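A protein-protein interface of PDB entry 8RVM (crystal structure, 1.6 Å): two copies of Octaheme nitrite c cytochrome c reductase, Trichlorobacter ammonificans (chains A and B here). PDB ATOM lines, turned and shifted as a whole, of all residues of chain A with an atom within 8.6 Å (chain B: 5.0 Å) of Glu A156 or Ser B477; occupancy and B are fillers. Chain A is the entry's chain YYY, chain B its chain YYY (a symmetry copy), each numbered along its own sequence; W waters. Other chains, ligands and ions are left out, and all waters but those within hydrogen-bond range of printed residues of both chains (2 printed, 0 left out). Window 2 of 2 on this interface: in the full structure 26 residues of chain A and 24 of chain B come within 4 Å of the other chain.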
ATOM      1  N   ASP A  90       3.825 -14.199 -16.056  1.00  0.00           N
ATOM      2  CA  ASP A  90       2.710 -13.267 -15.771  1.00  0.00           C
ATOM      3  C   ASP A  90       3.272 -11.832 -15.716  1.00  0.00           C
ATOM      4  O   ASP A  90       2.582 -10.924 -16.202  1.00  0.00           O
ATOM      5  CB  ASP A  90       1.971 -13.625 -14.492  1.00  0.00           C
ATOM      6  CG  ASP A  90       1.012 -14.787 -14.672  1.00  0.00           C
ATOM      7  OD1 ASP A  90       0.047 -14.655 -15.441  1.00  0.00           O
ATOM      8  OD2 ASP A  90       1.277 -15.830 -14.057  1.00  0.00           O
ATOM      9  N   GLY A  97      -2.407 -11.873 -23.985  1.00  0.00           N
ATOM     10  CA  GLY A  97      -3.403 -12.919 -23.708  1.00  0.00           C
ATOM     11  C   GLY A  97      -2.766 -14.194 -23.148  1.00  0.00           C
ATOM     12  O   GLY A  97      -3.488 -14.983 -22.553  1.00  0.00           O
ATOM     13  N   THR A  99      -1.079 -14.542 -20.668  1.00  0.00           N
ATOM     14  CA  THR A  99      -1.189 -14.488 -19.183  1.00  0.00           C
ATOM     15  C   THR A  99      -2.471 -15.202 -18.733  1.00  0.00           C
ATOM     16  O   THR A  99      -2.546 -15.561 -17.563  1.00  0.00           O
ATOM     17  CB  THR A  99      -1.067 -13.055 -18.633  1.00  0.00           C
ATOM     18  OG1 THR A  99      -2.218 -12.366 -19.123  1.00  0.00           O
ATOM     19  CG2 THR A  99       0.235 -12.394 -19.027  1.00  0.00           C
ATOM     20  N   PHE A 100      -3.431 -15.498 -19.617  1.00  0.00           N
ATOM     21  CA  PHE A 100      -4.694 -16.146 -19.201  1.00  0.00           C
ATOM     22  C   PHE A 100      -4.475 -17.660 -19.109  1.00  0.00           C
ATOM     23  O   PHE A 100      -4.987 -18.259 -18.153  1.00  0.00           O
ATOM     24  CB  PHE A 100      -5.839 -15.749 -20.120  1.00  0.00           C
ATOM     25  CG  PHE A 100      -6.266 -14.335 -19.848  1.00  0.00           C
ATOM     26  CD1 PHE A 100      -7.150 -14.058 -18.825  1.00  0.00           C
ATOM     27  CD2 PHE A 100      -5.681 -13.296 -20.539  1.00  0.00           C
ATOM     28  CE1 PHE A 100      -7.507 -12.736 -18.549  1.00  0.00           C
ATOM     29  CE2 PHE A 100      -6.038 -11.986 -20.268  1.00  0.00           C
ATOM     30  CZ  PHE A 100      -6.960 -11.716 -19.283  1.00  0.00           C
ATOM     31  N   GLU A 101      -3.715 -18.221 -20.036  1.00  0.00           N
ATOM     32  CA  GLU A 101      -3.283 -19.645 -19.948  1.00  0.00           C
ATOM     33  C   GLU A 101      -2.297 -19.925 -21.069  1.00  0.00           C
ATOM     34  O   GLU A 101      -2.578 -19.588 -22.250  1.00  0.00           O
ATOM     35  CB  GLU A 101      -4.416 -20.658 -20.015  1.00  0.00           C
ATOM     36  CG  GLU A 101      -3.909 -22.100 -19.920  1.00  0.00           C
ATOM     37  CD  GLU A 101      -5.004 -23.147 -19.849  1.00  0.00           C
ATOM     38  OE1 GLU A 101      -6.178 -22.820 -20.209  1.00  0.00           O
ATOM     39  OE2 GLU A 101      -4.677 -24.290 -19.461  1.00  0.00           O
ATOM     40  N   VAL A 118      -8.344 -24.088 -24.726  1.00  0.00           N
ATOM     41  CA  VAL A 118      -7.418 -23.283 -23.877  1.00  0.00           C
ATOM     42  C   VAL A 118      -8.159 -22.015 -23.429  1.00  0.00           C
ATOM     43  O   VAL A 118      -9.002 -21.494 -24.189  1.00  0.00           O
ATOM     44  CB  VAL A 118      -6.077 -22.956 -24.574  1.00  0.00           C
ATOM     45  CG1 VAL A 118      -6.230 -21.929 -25.679  1.00  0.00           C
ATOM     46  CG2 VAL A 118      -5.011 -22.506 -23.587  1.00  0.00           C
ATOM     47  N   ASP A 119      -7.847 -21.537 -22.232  1.00  0.00           N
ATOM     48  CA  ASP A 119      -8.590 -20.406 -21.621  1.00  0.00           C
ATOM     49  C   ASP A 119      -8.384 -19.142 -22.444  1.00  0.00           C
ATOM     50  O   ASP A 119      -9.183 -18.225 -22.245  1.00  0.00           O
ATOM     51  CB  ASP A 119      -8.177 -20.157 -20.189  1.00  0.00           C
ATOM     52  CG  ASP A 119      -8.691 -21.208 -19.229  1.00  0.00           C
ATOM     53  OD1 ASP A 119      -9.522 -22.036 -19.643  1.00  0.00           O
ATOM     54  OD2 ASP A 119      -8.237 -21.172 -18.091  1.00  0.00           O
ATOM     55  N   ARG A 120      -7.348 -19.062 -23.281  1.00  0.00           N
ATOM     56  CA  ARG A 120      -7.056 -17.824 -24.048  1.00  0.00           C
ATOM     57  C   ARG A 120      -7.763 -17.835 -25.410  1.00  0.00           C
ATOM     58  O   ARG A 120      -7.602 -16.805 -26.125  1.00  0.00           O
ATOM     59  CB  ARG A 120      -5.541 -17.580 -24.173  1.00  0.00           C
ATOM     60  CG  ARG A 120      -4.778 -18.562 -25.058  1.00  0.00           C
ATOM     61  CD  ARG A 120      -3.324 -18.154 -25.203  1.00  0.00           C
ATOM     62  NE  ARG A 120      -2.630 -18.940 -26.179  1.00  0.00           N
ATOM     63  CZ  ARG A 120      -2.076 -20.128 -25.955  1.00  0.00           C
ATOM     64  NH1 ARG A 120      -2.078 -20.672 -24.748  1.00  0.00           N
ATOM     65  NH2 ARG A 120      -1.496 -20.770 -26.944  1.00  0.00           N
ATOM     66  N   PHE A 121      -8.442 -18.925 -25.820  1.00  0.00           N
ATOM     67  CA  PHE A 121      -8.918 -19.075 -27.226  1.00  0.00           C
ATOM     68  C   PHE A 121     -10.212 -18.272 -27.484  1.00  0.00           C
ATOM     69  O   PHE A 121     -10.251 -17.406 -28.393  1.00  0.00           O
ATOM     70  CB  PHE A 121      -9.082 -20.554 -27.601  1.00  0.00           C
ATOM     71  CG  PHE A 121      -9.536 -20.791 -29.011  1.00  0.00           C
ATOM     72  CD1 PHE A 121      -8.709 -20.523 -30.095  1.00  0.00           C
ATOM     73  CD2 PHE A 121     -10.830 -21.204 -29.276  1.00  0.00           C
ATOM     74  CE1 PHE A 121      -9.139 -20.791 -31.392  1.00  0.00           C
ATOM     75  CE2 PHE A 121     -11.272 -21.422 -30.571  1.00  0.00           C
ATOM     76  CZ  PHE A 121     -10.425 -21.212 -31.629  1.00  0.00           C
ATOM     77  N   GLY A 123     -12.965 -17.404 -24.795  1.00  0.00           N
ATOM     78  CA  GLY A 123     -13.674 -17.067 -23.556  1.00  0.00           C
ATOM     79  C   GLY A 123     -14.221 -18.298 -22.852  1.00  0.00           C
ATOM     80  O   GLY A 123     -15.211 -18.179 -22.126  1.00  0.00           O
ATOM     81  N   GLY A 124     -13.588 -19.458 -23.055  1.00  0.00           N
ATOM     82  CA  GLY A 124     -13.987 -20.720 -22.427  1.00  0.00           C
ATOM     83  C   GLY A 124     -15.179 -21.352 -23.091  1.00  0.00           C
ATOM     84  O   GLY A 124     -15.807 -22.209 -22.469  1.00  0.00           O
ATOM     85  N   LYS A 153     -20.113 -17.088 -20.589  1.00  0.00           N
ATOM     86  CA  LYS A 153     -18.934 -16.368 -20.073  1.00  0.00           C
ATOM     87  C   LYS A 153     -18.178 -17.369 -19.204  1.00  0.00           C
ATOM     88  O   LYS A 153     -18.802 -18.314 -18.631  1.00  0.00           O
ATOM     89  CB  LYS A 153     -19.338 -15.119 -19.283  1.00  0.00           C
ATOM     90  CG  LYS A 153     -20.197 -14.105 -20.031  1.00  0.00           C
ATOM     91  CD  LYS A 153     -20.799 -13.033 -19.122  1.00  0.00           C
ATOM     92  CE  LYS A 153     -21.872 -12.189 -19.794  1.00  0.00           C
ATOM     93  NZ  LYS A 153     -21.985 -10.839 -19.190  1.00  0.00           N
ATOM     94  N   LEU A 154     -16.868 -17.263 -19.204  1.00  0.00           N
ATOM     95  CA  LEU A 154     -16.044 -18.048 -18.262  1.00  0.00           C
ATOM     96  C   LEU A 154     -15.007 -17.067 -17.735  1.00  0.00           C
ATOM     97  O   LEU A 154     -14.313 -16.457 -18.535  1.00  0.00           O
ATOM     98  CB  LEU A 154     -15.410 -19.208 -19.031  1.00  0.00           C
ATOM     99  CG  LEU A 154     -15.305 -20.555 -18.321  1.00  0.00           C
ATOM    100  CD1 LEU A 154     -13.978 -21.231 -18.642  1.00  0.00           C
ATOM    101  CD2 LEU A 154     -15.518 -20.469 -16.831  1.00  0.00           C
ATOM    102  N   PRO A 155     -14.944 -16.810 -16.412  1.00  0.00           N
ATOM    103  CA  PRO A 155     -14.010 -15.836 -15.865  1.00  0.00           C
ATOM    104  C   PRO A 155     -12.537 -16.112 -16.199  1.00  0.00           C
ATOM    105  O   PRO A 155     -12.133 -17.270 -16.280  1.00  0.00           O
ATOM    106  CB  PRO A 155     -14.242 -15.942 -14.356  1.00  0.00           C
ATOM    107  CG  PRO A 155     -15.641 -16.421 -14.242  1.00  0.00           C
ATOM    108  CD  PRO A 155     -15.780 -17.430 -15.366  1.00  0.00           C
ATOM    109  N   GLU A 156     -11.771 -15.032 -16.375  1.00  0.00           N
ATOM    110  CA  GLU A 156     -10.307 -15.071 -16.593  1.00  0.00           C
ATOM    111  C   GLU A 156     -10.022 -15.954 -17.815  1.00  0.00           C
ATOM    112  O   GLU A 156      -9.212 -16.889 -17.741  1.00  0.00           O
ATOM    113  CB  GLU A 156      -9.603 -15.516 -15.312  1.00  0.00           C
ATOM    114  CG  GLU A 156      -9.707 -14.489 -14.195  1.00  0.00           C
ATOM    115  CD  GLU A 156      -9.170 -13.116 -14.571  1.00  0.00           C
ATOM    116  OE1 GLU A 156      -8.133 -13.057 -15.268  1.00  0.00           O
ATOM    117  OE2 GLU A 156      -9.741 -12.108 -14.090  1.00  0.00           O
ATOM    118  N   THR A 157     -10.683 -15.644 -18.914  1.00  0.00           N
ATOM    119  CA  THR A 157     -10.368 -16.173 -20.256  1.00  0.00           C
ATOM    120  C   THR A 157     -10.012 -14.999 -21.169  1.00  0.00           C
ATOM    121  O   THR A 157     -10.138 -13.806 -20.743  1.00  0.00           O
ATOM    122  CB  THR A 157     -11.547 -16.977 -20.798  1.00  0.00           C
ATOM    123  OG1 THR A 157     -12.700 -16.133 -20.782  1.00  0.00           O
ATOM    124  CG2 THR A 157     -11.846 -18.226 -20.004  1.00  0.00           C
ATOM    125  N   ALA A 158      -9.611 -15.311 -22.391  1.00  0.00           N
ATOM    126  CA  ALA A 158      -9.345 -14.335 -23.459  1.00  0.00           C
ATOM    127  C   ALA A 158      -9.926 -14.835 -24.771  1.00  0.00           C
ATOM    128  O   ALA A 158     -10.420 -15.977 -24.825  1.00  0.00           O
ATOM    129  CB  ALA A 158      -7.874 -14.061 -23.597  1.00  0.00           C
ATOM    130  N   MET A 159      -9.846 -13.975 -25.784  1.00  0.00           N
ATOM    131  CA  MET A 159     -10.468 -14.191 -27.112  1.00  0.00           C
ATOM    132  C   MET A 159      -9.403 -14.064 -28.203  1.00  0.00           C
ATOM    133  O   MET A 159      -9.644 -13.349 -29.188  1.00  0.00           O
ATOM    134  CB  MET A 159     -11.578 -13.155 -27.310  1.00  0.00           C
ATOM    135  CG  MET A 159     -12.682 -13.273 -26.273  1.00  0.00           C
ATOM    136  SD  MET A 159     -13.831 -14.614 -26.640  1.00  0.00           S
ATOM    137  CE  MET A 159     -14.797 -13.866 -27.961  1.00  0.00           C
ATOM    138  N   LYS B 409      -3.610 -21.931 -11.831  1.00  0.00           N
ATOM    139  CA  LYS B 409      -4.509 -20.823 -11.375  1.00  0.00           C
ATOM    140  C   LYS B 409      -4.116 -20.428  -9.958  1.00  0.00           C
ATOM    141  O   LYS B 409      -4.206 -19.229  -9.613  1.00  0.00           O
ATOM    142  CB  LYS B 409      -5.970 -21.239 -11.510  1.00  0.00           C
ATOM    143  CG  LYS B 409      -6.387 -21.616 -12.911  1.00  0.00           C
ATOM    144  CD  LYS B 409      -6.054 -20.600 -13.997  1.00  0.00           C
ATOM    145  CE  LYS B 409      -6.581 -21.080 -15.325  1.00  0.00           C
ATOM    146  NZ  LYS B 409      -6.224 -20.207 -16.434  1.00  0.00           N
ATOM    147  N   ARG B 469     -11.541 -23.776  -9.846  1.00  0.00           N
ATOM    148  CA  ARG B 469     -11.352 -22.845 -10.976  1.00  0.00           C
ATOM    149  C   ARG B 469     -12.179 -21.583 -10.669  1.00  0.00           C
ATOM    150  O   ARG B 469     -11.643 -20.454 -10.796  1.00  0.00           O
ATOM    151  CB  ARG B 469     -11.699 -23.454 -12.337  1.00  0.00           C
ATOM    152  CG  ARG B 469     -11.335 -22.523 -13.489  1.00  0.00           C
ATOM    153  CD  ARG B 469     -11.932 -22.791 -14.861  1.00  0.00           C
ATOM    154  NE  ARG B 469     -11.195 -21.929 -15.781  1.00  0.00           N
ATOM    155  CZ  ARG B 469     -11.433 -20.613 -15.944  1.00  0.00           C
ATOM    156  NH1 ARG B 469     -12.466 -20.049 -15.347  1.00  0.00           N
ATOM    157  NH2 ARG B 469     -10.642 -19.886 -16.715  1.00  0.00           N
ATOM    158  N   THR B 473     -10.084 -18.141 -10.083  1.00  0.00           N
ATOM    159  CA  THR B 473     -10.248 -17.080 -11.109  1.00  0.00           C
ATOM    160  C   THR B 473     -10.937 -15.873 -10.466  1.00  0.00           C
ATOM    161  O   THR B 473     -10.587 -14.742 -10.865  1.00  0.00           O
ATOM    162  CB  THR B 473     -10.942 -17.588 -12.368  1.00  0.00           C
ATOM    163  OG1 THR B 473     -12.272 -18.022 -12.047  1.00  0.00           O
ATOM    164  CG2 THR B 473     -10.091 -18.651 -13.034  1.00  0.00           C
ATOM    165  N   GLY B 474     -11.850 -16.112  -9.531  1.00  0.00           N
ATOM    166  CA  GLY B 474     -12.487 -15.057  -8.715  1.00  0.00           C
ATOM    167  C   GLY B 474     -11.444 -14.300  -7.910  1.00  0.00           C
ATOM    168  O   GLY B 474     -11.547 -13.064  -7.784  1.00  0.00           O
ATOM    169  N   SER B 475     -10.471 -15.003  -7.338  1.00  0.00           N
ATOM    170  CA  SER B 475      -9.337 -14.382  -6.619  1.00  0.00           C
ATOM    171  C   SER B 475      -8.572 -13.449  -7.566  1.00  0.00           C
ATOM    172  O   SER B 475      -8.321 -12.280  -7.240  1.00  0.00           O
ATOM    173  CB  SER B 475      -8.456 -15.459  -6.019  1.00  0.00           C
ATOM    174  OG  SER B 475      -7.332 -14.875  -5.439  1.00  0.00           O
ATOM    175  N   ILE B 476      -8.154 -13.977  -8.716  1.00  0.00           N
ATOM    176  CA  ILE B 476      -7.391 -13.218  -9.739  1.00  0.00           C
ATOM    177  C   ILE B 476      -8.196 -11.971 -10.106  1.00  0.00           C
ATOM    178  O   ILE B 476      -7.571 -10.910 -10.221  1.00  0.00           O
ATOM    179  CB  ILE B 476      -7.117 -14.060 -10.993  1.00  0.00           C
ATOM    180  CG1 ILE B 476      -6.212 -15.228 -10.623  1.00  0.00           C
ATOM    181  CG2 ILE B 476      -6.529 -13.188 -12.095  1.00  0.00           C
ATOM    182  CD1 ILE B 476      -6.136 -16.358 -11.652  1.00  0.00           C
ATOM    183  N   SER B 477      -9.491 -12.140 -10.365  1.00  0.00           N
ATOM    184  CA  SER B 477     -10.394 -11.021 -10.791  1.00  0.00           C
ATOM    185  C   SER B 477     -10.394  -9.933  -9.709  1.00  0.00           C
ATOM    186  O   SER B 477     -10.239  -8.715 -10.086  1.00  0.00           O
ATOM    187  CB  SER B 477     -11.786 -11.475 -11.051  1.00  0.00           C
ATOM    188  OG  SER B 477     -11.853 -12.262 -12.209  1.00  0.00           O
ATOM    189  N   ALA B 478     -10.536 -10.336  -8.443  1.00  0.00           N
ATOM    190  CA  ALA B 478     -10.574  -9.403  -7.276  1.00  0.00           C
ATOM    191  C   ALA B 478      -9.239  -8.674  -7.169  1.00  0.00           C
ATOM    192  O   ALA B 478      -9.225  -7.434  -7.057  1.00  0.00           O
ATOM    193  CB  ALA B 478     -10.934 -10.095  -5.979  1.00  0.00           C
ATOM    194  N   SER B 479      -8.122  -9.385  -7.309  1.00  0.00           N
ATOM    195  CA  SER B 479      -6.786  -8.764  -7.173  1.00  0.00           C
ATOM    196  C   SER B 479      -6.584  -7.756  -8.312  1.00  0.00           C
ATOM    197  O   SER B 479      -6.073  -6.647  -8.062  1.00  0.00           O
ATOM    198  CB  SER B 479      -5.685  -9.775  -7.191  1.00  0.00           C
ATOM    199  OG  SER B 479      -5.684 -10.550  -6.016  1.00  0.00           O
ATOM    200  N   LYS B 480      -6.942  -8.138  -9.531  1.00  0.00           N
ATOM    201  CA  LYS B 480      -6.790  -7.258 -10.728  1.00  0.00           C
ATOM    202  C   LYS B 480      -7.629  -5.977 -10.551  1.00  0.00           C
ATOM    203  O   LYS B 480      -7.123  -4.864 -10.879  1.00  0.00           O
ATOM    204  CB  LYS B 480      -7.244  -8.015 -11.973  1.00  0.00           C
ATOM    205  CG  LYS B 480      -6.189  -8.934 -12.577  1.00  0.00           C
ATOM    206  CD  LYS B 480      -6.757  -9.664 -13.781  1.00  0.00           C
ATOM    207  CE  LYS B 480      -5.732 -10.505 -14.487  1.00  0.00           C
ATOM    208  NZ  LYS B 480      -6.285 -11.004 -15.760  1.00  0.00           N
ATOM    209  N   ALA B 481      -8.821  -6.107  -9.985  1.00  0.00           N
ATOM    210  CA  ALA B 481      -9.730  -4.974  -9.708  1.00  0.00           C
ATOM    211  C   ALA B 481      -9.119  -4.066  -8.635  1.00  0.00           C
ATOM    212  O   ALA B 481      -9.138  -2.834  -8.846  1.00  0.00           O
ATOM    213  CB  ALA B 481     -11.103  -5.470  -9.355  1.00  0.00           C
HETATM  214  O   HOH W   1      -4.199 -12.824 -16.646  1.00  0.00           O
HETATM  215  O   HOH W   2      -6.824 -17.455 -16.223  1.00  0.00           O
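Water W2 lies within hydrogen-bond range of the backbone carbonyl oxygen of Phe A100 (2.8 Å), the side-chain amino group of Lys B409 (2.8 Å) and the backbone carbonyl oxygen of Glu A156 (2.9 Å). Water W1 lies within hydrogen-bond range of NZ of Lys B480 (2.9 Å) and OG1 of Thr A99 (3.2 Å).
Glu A156 touches just these residues of chain B: Arg B469, Thr B473, Ile B476, Ser B477 and Lys B480. Ser B477 touches one residue of chain A. Printed residues of chain B within 4 Å of Asp A119: Lys B409 (2.8 Å) and Arg B469 (3.1 Å). Printed residues of chain B within 4 Å of Phe A100: Lys B409 and Lys B480. Asp A90 touches none of the printed residues of chain B. The nearest residue of chain B that does not touch Glu A156 is Lys B409 (4.7 Å). The nearest residue of chain A that does not touch Ser B477 is Pro A155 (4.9 Å).
Among the printed residues, pairs that only touch across the chains: Leu A154 with Arg B469 (3.4 Å), Glu A156 with Thr B473 (3.5 Å), Phe A100 with Lys B480 (3.5 Å), Glu A156 with Ile B476 (3.6 Å), Pro A155 with Thr B473 (3.7 Å) and Thr A157 with Arg B469 (3.9 Å).
The backbone carbonyl oxygen (O) of Asp A119 lies within hydrogen-bond range of the backbone NH (N) of Ala A158. O of Leu A154 lies within hydrogen-bond range of OG1 of Thr A157, 2.8 Å away. OG1 of Thr B473 sits at hydrogen-bond distance from O of Arg B469 (2.8 Å). O of Gly A123 sits close to N of Leu A154 (3.5 Å). OE1 of Glu A101 sits at hydrogen-bond distance from N of Asp A119. The backbone carbonyl oxygen (O) of Thr B473 is in hydrogen-bond range of the side-chain hydroxyl (OG) of Ser B477 (3.1 Å).
OD2 of Asp A119 lies within salt-bridge range of NZ of Lys B409 (2.8 Å). The backbone carbonyl oxygen (O) of Pro A155 sits at hydrogen-bond distance from the guanidinium group (NH1) of Arg B469 (3.0 Å). O of Glu A156 lies within hydrogen-bond range of NH2 of Arg B469 (3.5 Å). OE2 of Glu A156 sits at hydrogen-bond distance from OG of Ser B477. The side-chain carboxylate (OE1) of Glu A156 lies within salt-bridge range of the side-chain amino group (NZ) of Lys B480, at 2.8 Å. The side-chain amino group of Lys B409 sits at hydrogen-bond distance from the backbone carbonyl oxygen of Phe A100 (2.9 Å). The side-chain carboxylate (OD2) of Asp A119 lies within salt-bridge range of the guanidinium group (NH2) of Arg B469.
No position is printed for both chains. Of the 13 pairs that touch across the chains among the printed residues, none has its exchanged pair printed and touching as well.
Hydrophobic or aromatic side chains of chain A within 4 Å of the printed part of chain B: Phe A100, Leu A154 and Pro A155. Of the 11 printed residues of chain B, 6 touch a printed residue of chain A. Hydrophobic or aromatic side chains of chain B that line the printed part of chain A: Ile B476. Among the printed residues, 13 pairs touch across the chains. Among the printed residues, Asp or Glu carboxylates within 4 Å of a Lys or Arg side-chain nitrogen of the other chain: Asp A119 with Lys B409, Asp A119 with Arg B469 and Glu A156 with Lys B480.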
